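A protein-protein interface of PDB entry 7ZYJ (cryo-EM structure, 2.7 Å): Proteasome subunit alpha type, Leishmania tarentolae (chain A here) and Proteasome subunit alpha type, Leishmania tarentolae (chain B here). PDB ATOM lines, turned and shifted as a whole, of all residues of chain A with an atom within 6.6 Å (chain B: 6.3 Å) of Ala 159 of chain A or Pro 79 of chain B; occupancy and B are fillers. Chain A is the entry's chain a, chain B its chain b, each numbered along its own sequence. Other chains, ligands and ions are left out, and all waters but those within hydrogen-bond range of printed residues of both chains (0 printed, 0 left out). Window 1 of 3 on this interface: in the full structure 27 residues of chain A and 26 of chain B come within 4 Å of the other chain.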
ATOM      1  N   VAL A  22     -19.184  18.373 -11.809  1.00  0.00           N
ATOM      2  CA  VAL A  22     -19.348  19.587 -12.596  1.00  0.00           C
ATOM      3  C   VAL A  22     -20.485  19.450 -13.605  1.00  0.00           C
ATOM      4  O   VAL A  22     -21.183  20.429 -13.884  1.00  0.00           O
ATOM      5  CB  VAL A  22     -18.030  19.955 -13.293  1.00  0.00           C
ATOM      6  CG1 VAL A  22     -18.116  21.349 -13.866  1.00  0.00           C
ATOM      7  CG2 VAL A  22     -16.875  19.860 -12.314  1.00  0.00           C
ATOM      8  N   ALA A  25     -23.617  20.068 -11.632  1.00  0.00           N
ATOM      9  CA  ALA A  25     -23.850  21.487 -11.402  1.00  0.00           C
ATOM     10  C   ALA A  25     -24.442  22.174 -12.624  1.00  0.00           C
ATOM     11  O   ALA A  25     -25.093  23.214 -12.480  1.00  0.00           O
ATOM     12  CB  ALA A  25     -22.548  22.177 -10.994  1.00  0.00           C
ATOM     13  N   PHE A  26     -24.228  21.619 -13.818  1.00  0.00           N
ATOM     14  CA  PHE A  26     -24.880  22.155 -15.008  1.00  0.00           C
ATOM     15  C   PHE A  26     -26.374  21.868 -14.999  1.00  0.00           C
ATOM     16  O   PHE A  26     -27.156  22.648 -15.552  1.00  0.00           O
ATOM     17  CB  PHE A  26     -24.235  21.577 -16.266  1.00  0.00           C
ATOM     18  CG  PHE A  26     -23.133  22.426 -16.826  1.00  0.00           C
ATOM     19  CD1 PHE A  26     -23.408  23.658 -17.393  1.00  0.00           C
ATOM     20  CD2 PHE A  26     -21.819  21.992 -16.784  1.00  0.00           C
ATOM     21  CE1 PHE A  26     -22.395  24.440 -17.910  1.00  0.00           C
ATOM     22  CE2 PHE A  26     -20.801  22.771 -17.298  1.00  0.00           C
ATOM     23  CZ  PHE A  26     -21.089  23.996 -17.861  1.00  0.00           C
ATOM     24  N   GLY A 116     -14.242  32.990 -13.917  1.00  0.00           N
ATOM     25  CA  GLY A 116     -13.983  31.644 -14.391  1.00  0.00           C
ATOM     26  C   GLY A 116     -12.814  30.990 -13.685  1.00  0.00           C
ATOM     27  O   GLY A 116     -12.827  29.779 -13.447  1.00  0.00           O
ATOM     28  N   ASP A 117     -11.790  31.776 -13.348  1.00  0.00           N
ATOM     29  CA  ASP A 117     -10.694  31.259 -12.535  1.00  0.00           C
ATOM     30  C   ASP A 117     -11.188  30.815 -11.165  1.00  0.00           C
ATOM     31  O   ASP A 117     -10.760  29.776 -10.652  1.00  0.00           O
ATOM     32  CB  ASP A 117      -9.599  32.314 -12.388  1.00  0.00           C
ATOM     33  CG  ASP A 117      -8.760  32.463 -13.638  1.00  0.00           C
ATOM     34  OD1 ASP A 117      -8.817  31.568 -14.506  1.00  0.00           O
ATOM     35  OD2 ASP A 117      -8.039  33.474 -13.750  1.00  0.00           O
ATOM     36  N   ALA A 119     -14.193  29.726 -10.447  1.00  0.00           N
ATOM     37  CA  ALA A 119     -14.980  28.509 -10.615  1.00  0.00           C
ATOM     38  C   ALA A 119     -14.095  27.287 -10.818  1.00  0.00           C
ATOM     39  O   ALA A 119     -14.408  26.202 -10.317  1.00  0.00           O
ATOM     40  CB  ALA A 119     -15.946  28.668 -11.787  1.00  0.00           C
ATOM     41  N   GLN A 120     -12.990  27.443 -11.553  1.00  0.00           N
ATOM     42  CA  GLN A 120     -12.107  26.312 -11.818  1.00  0.00           C
ATOM     43  C   GLN A 120     -11.486  25.766 -10.540  1.00  0.00           C
ATOM     44  O   GLN A 120     -11.225  24.562 -10.444  1.00  0.00           O
ATOM     45  CB  GLN A 120     -11.016  26.722 -12.809  1.00  0.00           C
ATOM     46  CG  GLN A 120     -10.244  25.557 -13.411  1.00  0.00           C
ATOM     47  CD  GLN A 120      -9.052  25.143 -12.571  1.00  0.00           C
ATOM     48  OE1 GLN A 120      -8.662  25.842 -11.637  1.00  0.00           O
ATOM     49  NE2 GLN A 120      -8.467  23.998 -12.898  1.00  0.00           N
ATOM     50  N   THR A 123     -13.472  23.129  -8.910  1.00  0.00           N
ATOM     51  CA  THR A 123     -13.525  21.889  -9.670  1.00  0.00           C
ATOM     52  C   THR A 123     -12.251  21.065  -9.540  1.00  0.00           C
ATOM     53  O   THR A 123     -12.192  19.952 -10.071  1.00  0.00           O
ATOM     54  CB  THR A 123     -13.794  22.180 -11.149  1.00  0.00           C
ATOM     55  OG1 THR A 123     -12.651  22.817 -11.730  1.00  0.00           O
ATOM     56  CG2 THR A 123     -15.006  23.083 -11.300  1.00  0.00           C
ATOM     57  N   PRO A 130     -19.107  23.107  -6.540  1.00  0.00           N
ATOM     58  CA  PRO A 130     -19.264  24.137  -7.570  1.00  0.00           C
ATOM     59  C   PRO A 130     -20.582  24.876  -7.419  1.00  0.00           C
ATOM     60  O   PRO A 130     -21.568  24.343  -6.906  1.00  0.00           O
ATOM     61  CB  PRO A 130     -19.222  23.341  -8.882  1.00  0.00           C
ATOM     62  CG  PRO A 130     -18.608  22.025  -8.523  1.00  0.00           C
ATOM     63  CD  PRO A 130     -19.023  21.756  -7.115  1.00  0.00           C
ATOM     64  N   MET A 131     -20.588  26.127  -7.868  1.00  0.00           N
ATOM     65  CA  MET A 131     -21.792  26.948  -7.853  1.00  0.00           C
ATOM     66  C   MET A 131     -22.655  26.572  -9.050  1.00  0.00           C
ATOM     67  O   MET A 131     -22.249  26.766 -10.201  1.00  0.00           O
ATOM     68  CB  MET A 131     -21.436  28.433  -7.885  1.00  0.00           C
ATOM     69  CG  MET A 131     -20.664  28.926  -6.668  1.00  0.00           C
ATOM     70  SD  MET A 131     -21.675  29.108  -5.186  1.00  0.00           S
ATOM     71  CE  MET A 131     -21.376  27.548  -4.361  1.00  0.00           C
ATOM     72  N   VAL A 133     -24.748  27.683 -11.034  1.00  0.00           N
ATOM     73  CA  VAL A 133     -25.345  28.796 -11.758  1.00  0.00           C
ATOM     74  C   VAL A 133     -24.483  29.128 -12.967  1.00  0.00           C
ATOM     75  O   VAL A 133     -23.283  28.842 -12.999  1.00  0.00           O
ATOM     76  CB  VAL A 133     -25.520  30.050 -10.872  1.00  0.00           C
ATOM     77  CG1 VAL A 133     -26.510  29.789  -9.763  1.00  0.00           C
ATOM     78  CG2 VAL A 133     -24.188  30.476 -10.297  1.00  0.00           C
ATOM     79  N   VAL A 156     -20.047  32.867 -17.837  1.00  0.00           N
ATOM     80  CA  VAL A 156     -19.182  31.994 -17.056  1.00  0.00           C
ATOM     81  C   VAL A 156     -19.995  30.780 -16.631  1.00  0.00           C
ATOM     82  O   VAL A 156     -21.078  30.923 -16.050  1.00  0.00           O
ATOM     83  CB  VAL A 156     -18.597  32.715 -15.828  1.00  0.00           C
ATOM     84  CG1 VAL A 156     -17.621  31.807 -15.099  1.00  0.00           C
ATOM     85  CG2 VAL A 156     -17.917  34.007 -16.245  1.00  0.00           C
ATOM     86  N   ASP A 157     -19.475  29.595 -16.929  1.00  0.00           N
ATOM     87  CA  ASP A 157     -20.078  28.306 -16.628  1.00  0.00           C
ATOM     88  C   ASP A 157     -19.645  27.818 -15.253  1.00  0.00           C
ATOM     89  O   ASP A 157     -18.658  28.302 -14.691  1.00  0.00           O
ATOM     90  CB  ASP A 157     -19.678  27.287 -17.693  1.00  0.00           C
ATOM     91  CG  ASP A 157     -20.580  27.330 -18.910  1.00  0.00           C
ATOM     92  OD1 ASP A 157     -21.657  27.958 -18.832  1.00  0.00           O
ATOM     93  OD2 ASP A 157     -20.211  26.739 -19.947  1.00  0.00           O
ATOM     94  N   PRO A 158     -20.372  26.859 -14.673  1.00  0.00           N
ATOM     95  CA  PRO A 158     -19.897  26.239 -13.426  1.00  0.00           C
ATOM     96  C   PRO A 158     -18.568  25.521 -13.578  1.00  0.00           C
ATOM     97  O   PRO A 158     -17.883  25.297 -12.574  1.00  0.00           O
ATOM     98  CB  PRO A 158     -21.024  25.262 -13.065  1.00  0.00           C
ATOM     99  CG  PRO A 158     -22.225  25.795 -13.757  1.00  0.00           C
ATOM    100  CD  PRO A 158     -21.730  26.413 -15.027  1.00  0.00           C
ATOM    101  N   ALA A 159     -18.184  25.150 -14.802  1.00  0.00           N
ATOM    102  CA  ALA A 159     -16.892  24.519 -15.039  1.00  0.00           C
ATOM    103  C   ALA A 159     -15.753  25.523 -15.115  1.00  0.00           C
ATOM    104  O   ALA A 159     -14.592  25.115 -15.214  1.00  0.00           O
ATOM    105  CB  ALA A 159     -16.933  23.701 -16.331  1.00  0.00           C
ATOM    106  N   GLY A 160     -16.055  26.815 -15.071  1.00  0.00           N
ATOM    107  CA  GLY A 160     -15.054  27.841 -15.242  1.00  0.00           C
ATOM    108  C   GLY A 160     -14.820  28.276 -16.669  1.00  0.00           C
ATOM    109  O   GLY A 160     -13.859  29.009 -16.923  1.00  0.00           O
ATOM    110  N   TRP A 161     -15.661  27.848 -17.606  1.00  0.00           N
ATOM    111  CA  TRP A 161     -15.528  28.246 -19.001  1.00  0.00           C
ATOM    112  C   TRP A 161     -16.084  29.654 -19.166  1.00  0.00           C
ATOM    113  O   TRP A 161     -17.234  29.924 -18.808  1.00  0.00           O
ATOM    114  CB  TRP A 161     -16.251  27.259 -19.912  1.00  0.00           C
ATOM    115  CG  TRP A 161     -16.325  27.717 -21.335  1.00  0.00           C
ATOM    116  CD1 TRP A 161     -17.405  28.261 -21.964  1.00  0.00           C
ATOM    117  CD2 TRP A 161     -15.273  27.671 -22.306  1.00  0.00           C
ATOM    118  NE1 TRP A 161     -17.092  28.559 -23.268  1.00  0.00           N
ATOM    119  CE2 TRP A 161     -15.790  28.206 -23.503  1.00  0.00           C
ATOM    120  CE3 TRP A 161     -13.947  27.231 -22.279  1.00  0.00           C
ATOM    121  CZ2 TRP A 161     -15.026  28.312 -24.663  1.00  0.00           C
ATOM    122  CZ3 TRP A 161     -13.190  27.337 -23.433  1.00  0.00           C
ATOM    123  CH2 TRP A 161     -13.732  27.873 -24.608  1.00  0.00           C
ATOM    124  N   THR A 162     -15.270  30.552 -19.708  1.00  0.00           N
ATOM    125  CA  THR A 162     -15.651  31.939 -19.921  1.00  0.00           C
ATOM    126  C   THR A 162     -15.693  32.234 -21.413  1.00  0.00           C
ATOM    127  O   THR A 162     -14.773  31.878 -22.153  1.00  0.00           O
ATOM    128  CB  THR A 162     -14.667  32.884 -19.226  1.00  0.00           C
ATOM    129  OG1 THR A 162     -14.823  32.779 -17.806  1.00  0.00           O
ATOM    130  CG2 THR A 162     -14.904  34.322 -19.654  1.00  0.00           C
ATOM    131  N   TYR B  74      -3.249  24.425 -26.538  1.00  0.00           N
ATOM    132  CA  TYR B  74      -3.633  23.307 -25.690  1.00  0.00           C
ATOM    133  C   TYR B  74      -4.703  22.457 -26.361  1.00  0.00           C
ATOM    134  O   TYR B  74      -5.161  22.738 -27.472  1.00  0.00           O
ATOM    135  CB  TYR B  74      -4.133  23.800 -24.329  1.00  0.00           C
ATOM    136  CG  TYR B  74      -5.514  24.413 -24.369  1.00  0.00           C
ATOM    137  CD1 TYR B  74      -5.700  25.728 -24.774  1.00  0.00           C
ATOM    138  CD2 TYR B  74      -6.632  23.682 -23.991  1.00  0.00           C
ATOM    139  CE1 TYR B  74      -6.959  26.293 -24.810  1.00  0.00           C
ATOM    140  CE2 TYR B  74      -7.894  24.237 -24.026  1.00  0.00           C
ATOM    141  CZ  TYR B  74      -8.052  25.542 -24.435  1.00  0.00           C
ATOM    142  OH  TYR B  74      -9.310  26.099 -24.468  1.00  0.00           O
ATOM    143  N   GLY B  76      -8.016  20.018 -24.496  1.00  0.00           N
ATOM    144  CA  GLY B  76      -8.583  19.462 -23.284  1.00  0.00           C
ATOM    145  C   GLY B  76      -9.429  20.456 -22.518  1.00  0.00           C
ATOM    146  O   GLY B  76     -10.240  21.176 -23.108  1.00  0.00           O
ATOM    147  N   MET B  77      -9.250  20.507 -21.202  1.00  0.00           N
ATOM    148  CA  MET B  77     -10.024  21.406 -20.356  1.00  0.00           C
ATOM    149  C   MET B  77      -9.407  22.801 -20.383  1.00  0.00           C
ATOM    150  O   MET B  77      -8.294  23.004 -19.887  1.00  0.00           O
ATOM    151  CB  MET B  77     -10.085  20.869 -18.929  1.00  0.00           C
ATOM    152  CG  MET B  77     -10.798  19.534 -18.803  1.00  0.00           C
ATOM    153  SD  MET B  77     -10.960  18.981 -17.097  1.00  0.00           S
ATOM    154  CE  MET B  77     -12.212  17.714 -17.276  1.00  0.00           C
ATOM    155  N   GLY B  78     -10.130  23.756 -20.963  1.00  0.00           N
ATOM    156  CA  GLY B  78      -9.677  25.124 -21.054  1.00  0.00           C
ATOM    157  C   GLY B  78      -9.483  25.821 -19.721  1.00  0.00           C
ATOM    158  O   GLY B  78      -8.462  26.480 -19.490  1.00  0.00           O
ATOM    159  N   PRO B  79     -10.471  25.726 -18.823  1.00  0.00           N
ATOM    160  CA  PRO B  79     -10.276  26.287 -17.477  1.00  0.00           C
ATOM    161  C   PRO B  79      -9.086  25.694 -16.745  1.00  0.00           C
ATOM    162  O   PRO B  79      -8.402  26.416 -16.008  1.00  0.00           O
ATOM    163  CB  PRO B  79     -11.600  25.968 -16.762  1.00  0.00           C
ATOM    164  CG  PRO B  79     -12.369  25.073 -17.692  1.00  0.00           C
ATOM    165  CD  PRO B  79     -11.881  25.378 -19.059  1.00  0.00           C
ATOM    166  N   ASP B  80      -8.818  24.399 -16.921  1.00  0.00           N
ATOM    167  CA  ASP B  80      -7.596  23.817 -16.375  1.00  0.00           C
ATOM    168  C   ASP B  80      -6.364  24.435 -17.021  1.00  0.00           C
ATOM    169  O   ASP B  80      -5.362  24.692 -16.346  1.00  0.00           O
ATOM    170  CB  ASP B  80      -7.601  22.302 -16.571  1.00  0.00           C
ATOM    171  CG  ASP B  80      -8.101  21.556 -15.353  1.00  0.00           C
ATOM    172  OD1 ASP B  80      -8.461  22.215 -14.357  1.00  0.00           O
ATOM    173  OD2 ASP B  80      -8.134  20.309 -15.391  1.00  0.00           O
ATOM    174  N   CYS B  81      -6.424  24.676 -18.332  1.00  0.00           N
ATOM    175  CA  CYS B  81      -5.288  25.240 -19.050  1.00  0.00           C
ATOM    176  C   CYS B  81      -4.980  26.669 -18.632  1.00  0.00           C
ATOM    177  O   CYS B  81      -3.818  27.085 -18.681  1.00  0.00           O
ATOM    178  CB  CYS B  81      -5.545  25.197 -20.554  1.00  0.00           C
ATOM    179  SG  CYS B  81      -4.125  25.710 -21.524  1.00  0.00           S
ATOM    180  N   ARG B  82      -5.999  27.444 -18.255  1.00  0.00           N
ATOM    181  CA  ARG B  82      -5.771  28.860 -17.990  1.00  0.00           C
ATOM    182  C   ARG B  82      -4.893  29.059 -16.759  1.00  0.00           C
ATOM    183  O   ARG B  82      -4.097  30.005 -16.700  1.00  0.00           O
ATOM    184  CB  ARG B  82      -7.105  29.590 -17.833  1.00  0.00           C
ATOM    185  CG  ARG B  82      -6.968  31.100 -17.834  1.00  0.00           C
ATOM    186  CD  ARG B  82      -6.253  31.564 -19.095  1.00  0.00           C
ATOM    187  NE  ARG B  82      -6.030  33.004 -19.116  1.00  0.00           N
ATOM    188  CZ  ARG B  82      -6.844  33.880 -19.688  1.00  0.00           C
ATOM    189  NH1 ARG B  82      -7.953  33.496 -20.300  1.00  0.00           N
ATOM    190  NH2 ARG B  82      -6.536  35.174 -19.650  1.00  0.00           N
ATOM    191  N   VAL B  83      -5.015  28.170 -15.771  1.00  0.00           N
ATOM    192  CA  VAL B  83      -4.161  28.245 -14.588  1.00  0.00           C
ATOM    193  C   VAL B  83      -2.699  28.079 -14.981  1.00  0.00           C
ATOM    194  O   VAL B  83      -1.826  28.845 -14.551  1.00  0.00           O
ATOM    195  CB  VAL B  83      -4.588  27.189 -13.553  1.00  0.00           C
ATOM    196  CG1 VAL B  83      -3.681  27.237 -12.336  1.00  0.00           C
ATOM    197  CG2 VAL B  83      -6.040  27.390 -13.156  1.00  0.00           C
ATOM    198  N   LEU B  84      -2.413  27.078 -15.814  1.00  0.00           N
ATOM    199  CA  LEU B  84      -1.046  26.853 -16.266  1.00  0.00           C
ATOM    200  C   LEU B  84      -0.554  28.002 -17.136  1.00  0.00           C
ATOM    201  O   LEU B  84       0.623  28.368 -17.076  1.00  0.00           O
ATOM    202  CB  LEU B  84      -0.959  25.529 -17.020  1.00  0.00           C
ATOM    203  CG  LEU B  84      -1.358  24.305 -16.197  1.00  0.00           C
ATOM    204  CD1 LEU B  84      -1.779  23.171 -17.106  1.00  0.00           C
ATOM    205  CD2 LEU B  84      -0.215  23.872 -15.292  1.00  0.00           C
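Of the printed residues of chain B, Asp 117 of chain A touches Arg 82.
Of the printed residues of chain B, Gln 120 of chain A touches Pro 79, Asp 80 and Val 83.
Ala 159 of chain A touches just one residue of chain B: Pro 79 (3.3 Å).
Printed residues of chain B within 4 Å of Gly 160 of chain A: Pro 79 (3.8 Å).
Met 77 of chain B touches none of the printed residues of chain A.
Of chain A, only Gln 120, Ala 159 and Gly 160 come within 4 Å of Pro 79 of chain B.
Of the printed residues of chain A, Asp 80 of chain B touches Gln 120.
Of the printed residues of chain A, Arg 82 of chain B touches Asp 117.
The nearest printed residue of chain B that does not touch Asp 117 of chain A is Val 83 of chain B (5.2 Å).
O of Gln 120 of chain A sits at hydrogen-bond distance from OG1 of Thr 123 of chain A (2.6 Å).
The side-chain amide nitrogen (NE2) of Gln 120 of chain A sits close to the side-chain carboxylate (OD1) of Asp 80 of chain B (2.3 Å).
Along chain B the printed residues that touch a printed residue of chain A span positions 79 to 83.
Of the 18 printed residues of chain A, 4 touch a printed residue of chain B.
Among the printed residues, merely in contact across the chains: Gln 120 of chain A with Pro 79 of chain B, Ala 159 of chain A with Pro 79 of chain B, Gln 120 of chain A with Val 83 of chain B, Gly 160 of chain A with Pro 79 of chain B and Asp 117 of chain A with Arg 82 of chain B.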
